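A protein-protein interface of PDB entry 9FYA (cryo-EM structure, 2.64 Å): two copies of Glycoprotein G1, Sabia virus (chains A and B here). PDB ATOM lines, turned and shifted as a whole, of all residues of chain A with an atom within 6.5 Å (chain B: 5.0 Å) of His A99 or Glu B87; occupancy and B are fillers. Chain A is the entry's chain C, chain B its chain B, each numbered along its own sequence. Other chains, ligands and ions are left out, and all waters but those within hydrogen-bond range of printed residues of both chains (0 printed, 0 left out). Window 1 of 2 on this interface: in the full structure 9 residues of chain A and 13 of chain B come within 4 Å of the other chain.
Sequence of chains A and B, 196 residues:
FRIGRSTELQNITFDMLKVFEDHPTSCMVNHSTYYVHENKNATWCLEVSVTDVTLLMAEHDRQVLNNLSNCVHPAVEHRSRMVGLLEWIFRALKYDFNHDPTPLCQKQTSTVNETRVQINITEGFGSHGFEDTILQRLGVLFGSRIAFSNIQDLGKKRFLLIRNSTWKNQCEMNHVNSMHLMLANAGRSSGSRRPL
The side-chain carboxylate (OE1) of Glu B87 sits close to the side-chain hydroxyl (OG) of Ser A127, at 3.4 Å. NH2 of Arg B91 lies within salt-bridge range of OD2 of Asp A96, at 3.3 Å.
A ring nitrogen (ND1) of His A99 is in hydrogen-bond range of the side-chain carboxylate of Asp A96, 2.4 Å away. OE1 of Glu B87 lies within salt-bridge range of NH2 of Arg B91 (3.3 Å). OD2 of Asp A100 is in hydrogen-bond range of N of Asp A96, 2.7 Å away. NH1 of Arg B91 sits at hydrogen-bond distance from OD1 of Asn B185.
Phe B97 touches Asn A98 (CD1 to ND2, 3.4 Å). His A99 touches Glu B87. His A99 touches Phe B90. His A99 touches Phe B97. CG1 of Val B83 touches OG of Ser A127, 3.2 Å away. Ser A127 touches Gly B84 (OG to N, 3.997 Å).
Of the printed residues of chain B, Ser A127 touches Val B83, Gly B84 and Glu B87. Glu B87 touches two residues of chain A. Printed residues of chain A within 4 Å of Phe B97: Asn A98 and His A99. The nearest printed residue of chain A that does not touch Gly B84 is His A128 (4.7 Å).
Of the 13 printed residues of chain B, 6 touch a printed residue of chain A. Hydrophobic or aromatic side chains of chain B that line the printed part of chain A: Val B83, Phe B90 and Phe B97. Hydrophobic or aromatic side chains of chain A that line the printed part of chain B: His A99. Along chain A the printed residues that touch a printed residue of chain B span positions 96 to 127.
1 position is printed for both chains.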
ATOM      1  N   ASP A  96     -11.357   0.410  17.047  1.00  0.00           N
ATOM      2  CA  ASP A  96     -10.312  -0.022  16.123  1.00  0.00           C
ATOM      3  C   ASP A  96     -10.629  -1.439  15.661  1.00  0.00           C
ATOM      4  O   ASP A  96     -10.335  -2.410  16.356  1.00  0.00           O
ATOM      5  CB  ASP A  96      -8.949   0.061  16.799  1.00  0.00           C
ATOM      6  CG  ASP A  96      -7.807  -0.212  15.853  1.00  0.00           C
ATOM      7  OD1 ASP A  96      -8.003  -0.134  14.626  1.00  0.00           O
ATOM      8  OD2 ASP A  96      -6.696  -0.478  16.342  1.00  0.00           O
ATOM      9  N   PHE A  97     -11.244  -1.560  14.488  1.00  0.00           N
ATOM     10  CA  PHE A  97     -11.665  -2.871  14.015  1.00  0.00           C
ATOM     11  C   PHE A  97     -10.500  -3.770  13.618  1.00  0.00           C
ATOM     12  O   PHE A  97     -10.705  -4.974  13.451  1.00  0.00           O
ATOM     13  CB  PHE A  97     -12.650  -2.707  12.862  1.00  0.00           C
ATOM     14  CG  PHE A  97     -13.964  -2.121  13.286  1.00  0.00           C
ATOM     15  CD1 PHE A  97     -14.157  -0.751  13.294  1.00  0.00           C
ATOM     16  CD2 PHE A  97     -14.998  -2.937  13.700  1.00  0.00           C
ATOM     17  CE1 PHE A  97     -15.355  -0.213  13.690  1.00  0.00           C
ATOM     18  CE2 PHE A  97     -16.201  -2.398  14.097  1.00  0.00           C
ATOM     19  CZ  PHE A  97     -16.377  -1.034  14.092  1.00  0.00           C
ATOM     20  N   ASN A  98      -9.296  -3.223  13.449  1.00  0.00           N
ATOM     21  CA  ASN A  98      -8.137  -4.064  13.174  1.00  0.00           C
ATOM     22  C   ASN A  98      -7.596  -4.717  14.438  1.00  0.00           C
ATOM     23  O   ASN A  98      -7.124  -5.857  14.395  1.00  0.00           O
ATOM     24  CB  ASN A  98      -7.034  -3.253  12.493  1.00  0.00           C
ATOM     25  CG  ASN A  98      -7.509  -2.566  11.238  1.00  0.00           C
ATOM     26  OD1 ASN A  98      -7.839  -3.216  10.251  1.00  0.00           O
ATOM     27  ND2 ASN A  98      -7.536  -1.241  11.264  1.00  0.00           N
ATOM     28  N   HIS A  99      -7.650  -4.018  15.563  1.00  0.00           N
ATOM     29  CA  HIS A  99      -6.986  -4.458  16.779  1.00  0.00           C
ATOM     30  C   HIS A  99      -7.927  -4.759  17.931  1.00  0.00           C
ATOM     31  O   HIS A  99      -7.635  -5.657  18.719  1.00  0.00           O
ATOM     32  CB  HIS A  99      -5.965  -3.406  17.232  1.00  0.00           C
ATOM     33  CG  HIS A  99      -4.949  -3.070  16.188  1.00  0.00           C
ATOM     34  ND1 HIS A  99      -4.791  -1.797  15.686  1.00  0.00           N
ATOM     35  CD2 HIS A  99      -4.043  -3.842  15.546  1.00  0.00           C
ATOM     36  CE1 HIS A  99      -3.834  -1.801  14.778  1.00  0.00           C
ATOM     37  NE2 HIS A  99      -3.363  -3.029  14.674  1.00  0.00           N
ATOM     38  N   ASP A 100      -9.031  -4.032  18.062  1.00  0.00           N
ATOM     39  CA  ASP A 100      -9.928  -4.240  19.181  1.00  0.00           C
ATOM     40  C   ASP A 100     -10.633  -5.588  19.052  1.00  0.00           C
ATOM     41  O   ASP A 100     -10.750  -6.135  17.955  1.00  0.00           O
ATOM     42  CB  ASP A 100     -10.948  -3.110  19.258  1.00  0.00           C
ATOM     43  CG  ASP A 100     -10.315  -1.787  19.601  1.00  0.00           C
ATOM     44  OD1 ASP A 100      -9.143  -1.792  20.021  1.00  0.00           O
ATOM     45  OD2 ASP A 100     -10.983  -0.745  19.454  1.00  0.00           O
ATOM     46  N   PRO A 101     -11.097  -6.146  20.167  1.00  0.00           N
ATOM     47  CA  PRO A 101     -11.779  -7.443  20.116  1.00  0.00           C
ATOM     48  C   PRO A 101     -13.000  -7.408  19.209  1.00  0.00           C
ATOM     49  O   PRO A 101     -13.706  -6.403  19.111  1.00  0.00           O
ATOM     50  CB  PRO A 101     -12.175  -7.688  21.573  1.00  0.00           C
ATOM     51  CG  PRO A 101     -11.190  -6.928  22.346  1.00  0.00           C
ATOM     52  CD  PRO A 101     -10.867  -5.710  21.550  1.00  0.00           C
ATOM     53  N   THR A 102     -13.246  -8.526  18.552  1.00  0.00           N
ATOM     54  CA  THR A 102     -14.351  -8.619  17.612  1.00  0.00           C
ATOM     55  C   THR A 102     -15.681  -8.603  18.351  1.00  0.00           C
ATOM     56  O   THR A 102     -15.892  -9.431  19.246  1.00  0.00           O
ATOM     57  CB  THR A 102     -14.219  -9.886  16.777  1.00  0.00           C
ATOM     58  OG1 THR A 102     -13.015  -9.814  16.007  1.00  0.00           O
ATOM     59  CG2 THR A 102     -15.388 -10.024  15.833  1.00  0.00           C
ATOM     60  N   GLY A 126      -8.542  -8.370  25.373  1.00  0.00           N
ATOM     61  CA  GLY A 126      -7.954  -7.493  24.394  1.00  0.00           C
ATOM     62  C   GLY A 126      -6.547  -7.093  24.791  1.00  0.00           C
ATOM     63  O   GLY A 126      -5.957  -7.629  25.730  1.00  0.00           O
ATOM     64  N   SER A 127      -6.005  -6.137  24.047  1.00  0.00           N
ATOM     65  CA  SER A 127      -4.680  -5.641  24.364  1.00  0.00           C
ATOM     66  C   SER A 127      -4.701  -4.930  25.713  1.00  0.00           C
ATOM     67  O   SER A 127      -5.757  -4.669  26.293  1.00  0.00           O
ATOM     68  CB  SER A 127      -4.188  -4.690  23.277  1.00  0.00           C
ATOM     69  OG  SER A 127      -3.993  -5.374  22.061  1.00  0.00           O
ATOM     70  N   HIS A 128      -3.516  -4.618  26.219  1.00  0.00           N
ATOM     71  CA  HIS A 128      -3.429  -3.927  27.494  1.00  0.00           C
ATOM     72  C   HIS A 128      -4.095  -2.561  27.404  1.00  0.00           C
ATOM     73  O   HIS A 128      -3.874  -1.809  26.453  1.00  0.00           O
ATOM     74  CB  HIS A 128      -1.974  -3.773  27.917  1.00  0.00           C
ATOM     75  CG  HIS A 128      -1.810  -3.171  29.276  1.00  0.00           C
ATOM     76  ND1 HIS A 128      -1.332  -1.894  29.470  1.00  0.00           N
ATOM     77  CD2 HIS A 128      -2.070  -3.667  30.507  1.00  0.00           C
ATOM     78  CE1 HIS A 128      -1.308  -1.629  30.762  1.00  0.00           C
ATOM     79  NE2 HIS A 128      -1.749  -2.688  31.413  1.00  0.00           N
ATOM     80  N   LEU B  68      -3.057  -9.606  15.060  1.00  0.00           N
ATOM     81  CA  LEU B  68      -1.718  -9.226  15.502  1.00  0.00           C
ATOM     82  C   LEU B  68      -1.347  -9.871  16.831  1.00  0.00           C
ATOM     83  O   LEU B  68      -0.180 -10.213  17.049  1.00  0.00           O
ATOM     84  CB  LEU B  68      -1.627  -7.707  15.618  1.00  0.00           C
ATOM     85  CG  LEU B  68      -0.287  -7.095  16.007  1.00  0.00           C
ATOM     86  CD1 LEU B  68       0.792  -7.343  14.961  1.00  0.00           C
ATOM     87  CD2 LEU B  68      -0.462  -5.615  16.292  1.00  0.00           C
ATOM     88  N   VAL B  83       1.510  -6.524  22.714  1.00  0.00           N
ATOM     89  CA  VAL B  83       0.525  -6.335  21.649  1.00  0.00           C
ATOM     90  C   VAL B  83       0.007  -4.898  21.645  1.00  0.00           C
ATOM     91  O   VAL B  83      -0.193  -4.294  20.583  1.00  0.00           O
ATOM     92  CB  VAL B  83      -0.624  -7.354  21.793  1.00  0.00           C
ATOM     93  CG1 VAL B  83      -1.656  -7.157  20.703  1.00  0.00           C
ATOM     94  CG2 VAL B  83      -0.095  -8.768  21.735  1.00  0.00           C
ATOM     95  N   GLY B  84      -0.213  -4.328  22.830  1.00  0.00           N
ATOM     96  CA  GLY B  84      -0.614  -2.933  22.915  1.00  0.00           C
ATOM     97  C   GLY B  84       0.410  -1.982  22.326  1.00  0.00           C
ATOM     98  O   GLY B  84       0.058  -1.026  21.633  1.00  0.00           O
ATOM     99  N   LEU B  85       1.691  -2.212  22.621  1.00  0.00           N
ATOM    100  CA  LEU B  85       2.741  -1.368  22.063  1.00  0.00           C
ATOM    101  C   LEU B  85       2.850  -1.544  20.554  1.00  0.00           C
ATOM    102  O   LEU B  85       3.142  -0.586  19.831  1.00  0.00           O
ATOM    103  CB  LEU B  85       4.085  -1.676  22.724  1.00  0.00           C
ATOM    104  CG  LEU B  85       5.133  -0.557  22.723  1.00  0.00           C
ATOM    105  CD1 LEU B  85       4.560   0.747  23.253  1.00  0.00           C
ATOM    106  CD2 LEU B  85       6.396  -0.953  23.454  1.00  0.00           C
ATOM    107  N   LEU B  86       2.626  -2.763  20.062  1.00  0.00           N
ATOM    108  CA  LEU B  86       2.593  -2.990  18.622  1.00  0.00           C
ATOM    109  C   LEU B  86       1.480  -2.187  17.965  1.00  0.00           C
ATOM    110  O   LEU B  86       1.677  -1.592  16.900  1.00  0.00           O
ATOM    111  CB  LEU B  86       2.431  -4.480  18.329  1.00  0.00           C
ATOM    112  CG  LEU B  86       3.699  -5.326  18.436  1.00  0.00           C
ATOM    113  CD1 LEU B  86       3.364  -6.796  18.490  1.00  0.00           C
ATOM    114  CD2 LEU B  86       4.633  -5.037  17.278  1.00  0.00           C
ATOM    115  N   GLU B  87       0.299  -2.166  18.584  1.00  0.00           N
ATOM    116  CA  GLU B  87      -0.798  -1.355  18.065  1.00  0.00           C
ATOM    117  C   GLU B  87      -0.474   0.132  18.127  1.00  0.00           C
ATOM    118  O   GLU B  87      -0.851   0.894  17.231  1.00  0.00           O
ATOM    119  CB  GLU B  87      -2.080  -1.662  18.828  1.00  0.00           C
ATOM    120  CG  GLU B  87      -2.486  -3.106  18.753  1.00  0.00           C
ATOM    121  CD  GLU B  87      -3.558  -3.457  19.743  1.00  0.00           C
ATOM    122  OE1 GLU B  87      -4.195  -2.533  20.279  1.00  0.00           O
ATOM    123  OE2 GLU B  87      -3.782  -4.659  19.968  1.00  0.00           O
ATOM    124  N   TRP B  88       0.201   0.570  19.192  1.00  0.00           N
ATOM    125  CA  TRP B  88       0.629   1.963  19.273  1.00  0.00           C
ATOM    126  C   TRP B  88       1.579   2.322  18.138  1.00  0.00           C
ATOM    127  O   TRP B  88       1.464   3.393  17.538  1.00  0.00           O
ATOM    128  CB  TRP B  88       1.267   2.239  20.630  1.00  0.00           C
ATOM    129  CG  TRP B  88       0.293   2.707  21.660  1.00  0.00           C
ATOM    130  CD1 TRP B  88      -0.807   2.049  22.103  1.00  0.00           C
ATOM    131  CD2 TRP B  88       0.352   3.932  22.393  1.00  0.00           C
ATOM    132  NE1 TRP B  88      -1.452   2.792  23.054  1.00  0.00           N
ATOM    133  CE2 TRP B  88      -0.756   3.953  23.256  1.00  0.00           C
ATOM    134  CE3 TRP B  88       1.231   5.015  22.400  1.00  0.00           C
ATOM    135  CZ2 TRP B  88      -1.009   5.015  24.116  1.00  0.00           C
ATOM    136  CZ3 TRP B  88       0.976   6.065  23.246  1.00  0.00           C
ATOM    137  CH2 TRP B  88      -0.133   6.061  24.093  1.00  0.00           C
ATOM    138  N   ILE B  89       2.528   1.438  17.832  1.00  0.00           N
ATOM    139  CA  ILE B  89       3.443   1.676  16.719  1.00  0.00           C
ATOM    140  C   ILE B  89       2.677   1.720  15.406  1.00  0.00           C
ATOM    141  O   ILE B  89       2.920   2.577  14.549  1.00  0.00           O
ATOM    142  CB  ILE B  89       4.543   0.602  16.684  1.00  0.00           C
ATOM    143  CG1 ILE B  89       5.463   0.729  17.894  1.00  0.00           C
ATOM    144  CG2 ILE B  89       5.334   0.683  15.387  1.00  0.00           C
ATOM    145  CD1 ILE B  89       6.387  -0.426  18.050  1.00  0.00           C
ATOM    146  N   PHE B  90       1.747   0.786  15.228  1.00  0.00           N
ATOM    147  CA  PHE B  90       0.999   0.682  13.983  1.00  0.00           C
ATOM    148  C   PHE B  90       0.151   1.926  13.745  1.00  0.00           C
ATOM    149  O   PHE B  90       0.056   2.417  12.616  1.00  0.00           O
ATOM    150  CB  PHE B  90       0.121  -0.561  14.059  1.00  0.00           C
ATOM    151  CG  PHE B  90       0.825  -1.810  13.653  1.00  0.00           C
ATOM    152  CD1 PHE B  90       2.128  -1.765  13.217  1.00  0.00           C
ATOM    153  CD2 PHE B  90       0.226  -3.041  13.803  1.00  0.00           C
ATOM    154  CE1 PHE B  90       2.796  -2.913  12.871  1.00  0.00           C
ATOM    155  CE2 PHE B  90       0.897  -4.192  13.454  1.00  0.00           C
ATOM    156  CZ  PHE B  90       2.181  -4.124  12.990  1.00  0.00           C
ATOM    157  N   ARG B  91      -0.488   2.439  14.799  1.00  0.00           N
ATOM    158  CA  ARG B  91      -1.257   3.672  14.695  1.00  0.00           C
ATOM    159  C   ARG B  91      -0.356   4.884  14.536  1.00  0.00           C
ATOM    160  O   ARG B  91      -0.753   5.875  13.913  1.00  0.00           O
ATOM    161  CB  ARG B  91      -2.134   3.847  15.931  1.00  0.00           C
ATOM    162  CG  ARG B  91      -3.362   2.971  15.963  1.00  0.00           C
ATOM    163  CD  ARG B  91      -4.244   3.309  17.152  1.00  0.00           C
ATOM    164  NE  ARG B  91      -4.890   2.120  17.693  1.00  0.00           N
ATOM    165  CZ  ARG B  91      -4.479   1.457  18.764  1.00  0.00           C
ATOM    166  NH1 ARG B  91      -3.419   1.843  19.452  1.00  0.00           N
ATOM    167  NH2 ARG B  91      -5.141   0.372  19.144  1.00  0.00           N
ATOM    168  N   ALA B  92       0.854   4.831  15.097  1.00  0.00           N
ATOM    169  CA  ALA B  92       1.807   5.917  14.913  1.00  0.00           C
ATOM    170  C   ALA B  92       2.342   5.962  13.491  1.00  0.00           C
ATOM    171  O   ALA B  92       2.631   7.044  12.977  1.00  0.00           O
ATOM    172  CB  ALA B  92       2.948   5.784  15.916  1.00  0.00           C
ATOM    173  N   PHE B  97      -4.709  -0.316   6.791  1.00  0.00           N
ATOM    174  CA  PHE B  97      -4.856  -1.758   6.657  1.00  0.00           C
ATOM    175  C   PHE B  97      -5.717  -2.167   5.468  1.00  0.00           C
ATOM    176  O   PHE B  97      -5.699  -3.343   5.095  1.00  0.00           O
ATOM    177  CB  PHE B  97      -5.400  -2.340   7.957  1.00  0.00           C
ATOM    178  CG  PHE B  97      -4.425  -2.262   9.096  1.00  0.00           C
ATOM    179  CD1 PHE B  97      -4.387  -1.153   9.920  1.00  0.00           C
ATOM    180  CD2 PHE B  97      -3.529  -3.287   9.324  1.00  0.00           C
ATOM    181  CE1 PHE B  97      -3.491  -1.077  10.957  1.00  0.00           C
ATOM    182  CE2 PHE B  97      -2.629  -3.213  10.365  1.00  0.00           C
ATOM    183  CZ  PHE B  97      -2.612  -2.105  11.181  1.00  0.00           C
ATOM    184  N   ASN B 185      -1.791   8.300  19.010  1.00  0.00           N
ATOM    185  CA  ASN B 185      -2.642   7.401  19.776  1.00  0.00           C
ATOM    186  C   ASN B 185      -3.474   8.163  20.797  1.00  0.00           C
ATOM    187  O   ASN B 185      -3.621   7.738  21.941  1.00  0.00           O
ATOM    188  CB  ASN B 185      -1.812   6.329  20.478  1.00  0.00           C
ATOM    189  CG  ASN B 185      -1.057   5.450  19.513  1.00  0.00           C
ATOM    190  OD1 ASN B 185      -1.545   4.406  19.101  1.00  0.00           O
ATOM    191  ND2 ASN B 185       0.154   5.859  19.165  1.00  0.00           N
